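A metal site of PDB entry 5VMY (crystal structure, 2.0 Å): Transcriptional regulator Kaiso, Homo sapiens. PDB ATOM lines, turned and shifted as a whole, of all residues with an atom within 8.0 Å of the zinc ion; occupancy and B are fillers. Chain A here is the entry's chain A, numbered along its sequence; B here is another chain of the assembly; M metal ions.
ND1 of His 42 sits close to OH of Tyr 33, 3.0 Å away.
The side-chain sulfur of Cys 29 sits close to the backbone NH of Arg 31.
SG of Cys 26 lies close to N of Val 28, at 3.3 Å.
N of Cys 26 is in hydrogen-bond range of O of Arg 31, at 2.9 Å.
The zinc ion is bound by NE2 of His 46 (2.0 Å), NE2 of His 42 (2.1 Å), SG of Cys 29 (2.2 Å) and SG of Cys 26 (2.3 Å).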
ATOM      1  N   ASP A  12       4.259 -19.751   7.965  1.00  0.00           N
ATOM      2  CA  ASP A  12       4.010 -21.186   7.807  1.00  0.00           C
ATOM      3  C   ASP A  12       3.213 -21.492   6.544  1.00  0.00           C
ATOM      4  O   ASP A  12       2.898 -22.652   6.266  1.00  0.00           O
ATOM      5  CB  ASP A  12       3.277 -21.749   9.039  1.00  0.00           C
ATOM      6  CG  ASP A  12       1.929 -21.110   9.256  1.00  0.00           C
ATOM      7  OD1 ASP A  12       1.659 -20.047   8.660  1.00  0.00           O
ATOM      8  OD2 ASP A  12       1.115 -21.671  10.043  1.00  0.00           O
ATOM      9  N   ILE A  25      -1.730 -22.244   1.461  1.00  0.00           N
ATOM     10  CA  ILE A  25      -0.907 -23.404   1.131  1.00  0.00           C
ATOM     11  C   ILE A  25       0.159 -23.637   2.180  1.00  0.00           C
ATOM     12  O   ILE A  25       0.932 -22.738   2.486  1.00  0.00           O
ATOM     13  CB  ILE A  25      -0.199 -23.262  -0.252  1.00  0.00           C
ATOM     14  CG1 ILE A  25      -1.181 -23.473  -1.397  1.00  0.00           C
ATOM     15  CG2 ILE A  25       0.878 -24.304  -0.389  1.00  0.00           C
ATOM     16  CD1 ILE A  25      -2.133 -22.339  -1.600  1.00  0.00           C
ATOM     17  N   CYS A  26       0.199 -24.847   2.718  1.00  0.00           N
ATOM     18  CA  CYS A  26       1.212 -25.221   3.686  1.00  0.00           C
ATOM     19  C   CYS A  26       2.593 -25.173   3.048  1.00  0.00           C
ATOM     20  O   CYS A  26       2.849 -25.841   2.048  1.00  0.00           O
ATOM     21  CB  CYS A  26       0.948 -26.621   4.237  1.00  0.00           C
ATOM     22  SG  CYS A  26       2.272 -27.183   5.281  1.00  0.00           S
ATOM     23  N   ILE A  27       3.499 -24.385   3.632  1.00  0.00           N
ATOM     24  CA  ILE A  27       4.819 -24.220   3.040  1.00  0.00           C
ATOM     25  C   ILE A  27       5.589 -25.543   3.085  1.00  0.00           C
ATOM     26  O   ILE A  27       6.499 -25.747   2.301  1.00  0.00           O
ATOM     27  CB  ILE A  27       5.618 -23.095   3.752  1.00  0.00           C
ATOM     28  CG1 ILE A  27       6.913 -22.791   2.987  1.00  0.00           C
ATOM     29  CG2 ILE A  27       5.939 -23.475   5.172  1.00  0.00           C
ATOM     30  CD1 ILE A  27       6.719 -22.598   1.509  1.00  0.00           C
ATOM     31  N   VAL A  28       5.216 -26.453   3.979  1.00  0.00           N
ATOM     32  CA  VAL A  28       5.959 -27.702   4.069  1.00  0.00           C
ATOM     33  C   VAL A  28       5.499 -28.754   3.052  1.00  0.00           C
ATOM     34  O   VAL A  28       6.294 -29.197   2.235  1.00  0.00           O
ATOM     35  CB  VAL A  28       5.873 -28.286   5.494  1.00  0.00           C
ATOM     36  CG1 VAL A  28       6.391 -29.719   5.509  1.00  0.00           C
ATOM     37  CG2 VAL A  28       6.649 -27.410   6.470  1.00  0.00           C
ATOM     38  N   CYS A  29       4.227 -29.154   3.090  1.00  0.00           N
ATOM     39  CA  CYS A  29       3.752 -30.216   2.199  1.00  0.00           C
ATOM     40  C   CYS A  29       2.880 -29.725   1.031  1.00  0.00           C
ATOM     41  O   CYS A  29       2.414 -30.530   0.230  1.00  0.00           O
ATOM     42  CB  CYS A  29       2.969 -31.257   2.998  1.00  0.00           C
ATOM     43  SG  CYS A  29       1.476 -30.632   3.786  1.00  0.00           S
ATOM     44  N   LYS A  30       2.663 -28.410   0.960  1.00  0.00           N
ATOM     45  CA  LYS A  30       1.863 -27.783  -0.089  1.00  0.00           C
ATOM     46  C   LYS A  30       0.383 -28.194  -0.092  1.00  0.00           C
ATOM     47  O   LYS A  30      -0.276 -28.157  -1.127  1.00  0.00           O
ATOM     48  CB  LYS A  30       2.456 -28.072  -1.476  1.00  0.00           C
ATOM     49  CG  LYS A  30       3.943 -27.769  -1.616  1.00  0.00           C
ATOM     50  CD  LYS A  30       4.197 -26.272  -1.577  1.00  0.00           C
ATOM     51  CE  LYS A  30       5.662 -25.960  -1.891  1.00  0.00           C
ATOM     52  NZ  LYS A  30       6.575 -26.629  -0.917  1.00  0.00           N
ATOM     53  N   ARG A  31      -0.155 -28.574   1.060  1.00  0.00           N
ATOM     54  CA  ARG A  31      -1.592 -28.839   1.111  1.00  0.00           C
ATOM     55  C   ARG A  31      -2.352 -27.524   1.071  1.00  0.00           C
ATOM     56  O   ARG A  31      -1.896 -26.544   1.660  1.00  0.00           O
ATOM     57  CB  ARG A  31      -1.975 -29.638   2.378  1.00  0.00           C
ATOM     58  CG  ARG A  31      -1.872 -31.135   2.212  1.00  0.00           C
ATOM     59  CD  ARG A  31      -2.077 -31.860   3.530  1.00  0.00           C
ATOM     60  NE  ARG A  31      -1.898 -33.298   3.404  1.00  0.00           N
ATOM     61  CZ  ARG A  31      -2.880 -34.151   3.097  1.00  0.00           C
ATOM     62  NH1 ARG A  31      -4.115 -33.698   2.874  1.00  0.00           N
ATOM     63  NH2 ARG A  31      -2.618 -35.438   3.005  1.00  0.00           N
ATOM     64  N   SER A  32      -3.497 -27.507   0.404  1.00  0.00           N
ATOM     65  CA  SER A  32      -4.292 -26.284   0.279  1.00  0.00           C
ATOM     66  C   SER A  32      -5.481 -26.260   1.235  1.00  0.00           C
ATOM     67  O   SER A  32      -6.141 -27.276   1.466  1.00  0.00           O
ATOM     68  CB  SER A  32      -4.796 -26.103  -1.158  1.00  0.00           C
ATOM     69  OG  SER A  32      -5.659 -27.151  -1.542  1.00  0.00           O
ATOM     70  N   TYR A  33      -5.737 -25.083   1.794  1.00  0.00           N
ATOM     71  CA  TYR A  33      -6.808 -24.903   2.755  1.00  0.00           C
ATOM     72  C   TYR A  33      -7.654 -23.689   2.404  1.00  0.00           C
ATOM     73  O   TYR A  33      -7.124 -22.641   2.007  1.00  0.00           O
ATOM     74  CB  TYR A  33      -6.235 -24.792   4.184  1.00  0.00           C
ATOM     75  CG  TYR A  33      -5.520 -26.061   4.563  1.00  0.00           C
ATOM     76  CD1 TYR A  33      -4.160 -26.241   4.290  1.00  0.00           C
ATOM     77  CD2 TYR A  33      -6.222 -27.125   5.133  1.00  0.00           C
ATOM     78  CE1 TYR A  33      -3.529 -27.434   4.606  1.00  0.00           C
ATOM     79  CE2 TYR A  33      -5.601 -28.309   5.445  1.00  0.00           C
ATOM     80  CZ  TYR A  33      -4.255 -28.469   5.194  1.00  0.00           C
ATOM     81  OH  TYR A  33      -3.634 -29.654   5.506  1.00  0.00           O
ATOM     82  N   LEU A  39      -5.288 -24.534   8.138  1.00  0.00           N
ATOM     83  CA  LEU A  39      -3.872 -24.686   7.870  1.00  0.00           C
ATOM     84  C   LEU A  39      -3.137 -24.751   9.201  1.00  0.00           C
ATOM     85  O   LEU A  39      -2.255 -25.586   9.403  1.00  0.00           O
ATOM     86  CB  LEU A  39      -3.333 -23.550   7.020  1.00  0.00           C
ATOM     87  CG  LEU A  39      -1.850 -23.718   6.701  1.00  0.00           C
ATOM     88  CD1 LEU A  39      -1.614 -23.466   5.228  1.00  0.00           C
ATOM     89  CD2 LEU A  39      -1.033 -22.771   7.554  1.00  0.00           C
ATOM     90  N   HIS A  42      -3.609 -28.040  10.891  1.00  0.00           N
ATOM     91  CA  HIS A  42      -2.809 -28.998  10.169  1.00  0.00           C
ATOM     92  C   HIS A  42      -1.313 -28.847  10.456  1.00  0.00           C
ATOM     93  O   HIS A  42      -0.591 -29.836  10.621  1.00  0.00           O
ATOM     94  CB  HIS A  42      -3.040 -28.847   8.658  1.00  0.00           C
ATOM     95  CG  HIS A  42      -1.916 -29.391   7.839  1.00  0.00           C
ATOM     96  ND1 HIS A  42      -1.733 -30.741   7.620  1.00  0.00           N
ATOM     97  CD2 HIS A  42      -0.888 -28.767   7.213  1.00  0.00           C
ATOM     98  CE1 HIS A  42      -0.653 -30.915   6.867  1.00  0.00           C
ATOM     99  NE2 HIS A  42      -0.120 -29.731   6.618  1.00  0.00           N
ATOM    100  N   PHE A  43      -0.841 -27.608  10.532  1.00  0.00           N
ATOM    101  CA  PHE A  43       0.602 -27.364  10.542  1.00  0.00           C
ATOM    102  C   PHE A  43       1.279 -27.961  11.776  1.00  0.00           C
ATOM    103  O   PHE A  43       2.476 -28.262  11.746  1.00  0.00           O
ATOM    104  CB  PHE A  43       0.898 -25.869  10.459  1.00  0.00           C
ATOM    105  CG  PHE A  43       2.312 -25.562  10.058  1.00  0.00           C
ATOM    106  CD1 PHE A  43       2.695 -25.601   8.730  1.00  0.00           C
ATOM    107  CD2 PHE A  43       3.267 -25.215  11.005  1.00  0.00           C
ATOM    108  CE1 PHE A  43       3.989 -25.317   8.347  1.00  0.00           C
ATOM    109  CE2 PHE A  43       4.567 -24.930  10.630  1.00  0.00           C
ATOM    110  CZ  PHE A  43       4.931 -24.976   9.292  1.00  0.00           C
ATOM    111  N   ASN A  44       0.514 -28.166  12.848  1.00  0.00           N
ATOM    112  CA  ASN A  44       1.072 -28.738  14.073  1.00  0.00           C
ATOM    113  C   ASN A  44       1.665 -30.122  13.852  1.00  0.00           C
ATOM    114  O   ASN A  44       2.561 -30.542  14.568  1.00  0.00           O
ATOM    115  CB  ASN A  44       0.014 -28.808  15.170  1.00  0.00           C
ATOM    116  CG  ASN A  44       0.623 -28.862  16.548  1.00  0.00           C
ATOM    117  OD1 ASN A  44       1.509 -28.065  16.868  1.00  0.00           O
ATOM    118  ND2 ASN A  44       0.193 -29.818  17.360  1.00  0.00           N
ATOM    119  N   ILE A  45       1.142 -30.831  12.852  1.00  0.00           N
ATOM    120  CA  ILE A  45       1.696 -32.121  12.431  1.00  0.00           C
ATOM    121  C   ILE A  45       3.175 -31.996  12.033  1.00  0.00           C
ATOM    122  O   ILE A  45       3.979 -32.887  12.271  1.00  0.00           O
ATOM    123  CB  ILE A  45       0.890 -32.695  11.256  1.00  0.00           C
ATOM    124  CG1 ILE A  45      -0.555 -32.985  11.694  1.00  0.00           C
ATOM    125  CG2 ILE A  45       1.524 -33.964  10.708  1.00  0.00           C
ATOM    126  CD1 ILE A  45      -1.489 -33.340  10.553  1.00  0.00           C
ATOM    127  N   HIS A  46       3.523 -30.863  11.421  1.00  0.00           N
ATOM    128  CA  HIS A  46       4.906 -30.606  11.044  1.00  0.00           C
ATOM    129  C   HIS A  46       5.756 -30.090  12.211  1.00  0.00           C
ATOM    130  O   HIS A  46       6.887 -30.530  12.414  1.00  0.00           O
ATOM    131  CB  HIS A  46       4.981 -29.599   9.900  1.00  0.00           C
ATOM    132  CG  HIS A  46       4.238 -30.023   8.674  1.00  0.00           C
ATOM    133  ND1 HIS A  46       4.371 -31.282   8.124  1.00  0.00           N
ATOM    134  CD2 HIS A  46       3.385 -29.341   7.867  1.00  0.00           C
ATOM    135  CE1 HIS A  46       3.617 -31.360   7.039  1.00  0.00           C
ATOM    136  NE2 HIS A  46       3.014 -30.204   6.854  1.00  0.00           N
ATOM    137  N1  5CM B   8     -11.093 -31.071   7.840  1.00  0.00           N
ATOM    138  C2  5CM B   8     -12.402 -31.705   8.026  1.00  0.00           C
ATOM    139  N3  5CM B   8     -12.614 -32.518   9.224  1.00  0.00           N
ATOM    140  C4  5CM B   8     -11.571 -32.725  10.176  1.00  0.00           C
ATOM    141  C5  5CM B   8     -10.251 -32.099   9.995  1.00  0.00           C
ATOM    142  C5A 5CM B   8      -9.172 -32.327  11.047  1.00  0.00           C
ATOM    143  C6  5CM B   8     -10.015 -31.253   8.804  1.00  0.00           C
ATOM    144  O2  5CM B   8     -13.282 -31.541   7.251  1.00  0.00           O
ATOM    145  N4  5CM B   8     -11.839 -33.550  11.329  1.00  0.00           N
ATOM    146  C1' 5CM B   8     -10.923 -30.266   6.638  1.00  0.00           C
ATOM    147  C2' 5CM B   8      -9.682 -29.302   6.677  1.00  0.00           C
ATOM    148  C3' 5CM B   8      -9.597 -29.007   5.195  1.00  0.00           C
ATOM    149  C4' 5CM B   8      -9.853 -30.199   4.593  1.00  0.00           C
ATOM    150  O4' 5CM B   8     -10.598 -31.102   5.701  1.00  0.00           O
ATOM    151  O3' 5CM B   8     -10.776 -28.144   4.920  1.00  0.00           O
ATOM    152  C5' 5CM B   8      -8.646 -30.926   4.106  1.00  0.00           C
ATOM    153  O5' 5CM B   8      -7.737 -31.041   5.162  1.00  0.00           O
ATOM    154  P   5CM B   8      -6.377 -31.933   4.903  1.00  0.00           P
ATOM    155  OP1 5CM B   8      -5.920 -31.780   3.488  1.00  0.00           O
ATOM    156  OP2 5CM B   8      -5.331 -31.582   5.931  1.00  0.00           O
HETATM  157 ZN    ZN M   1       1.700 -29.417   5.619  1.00  0.00          ZN
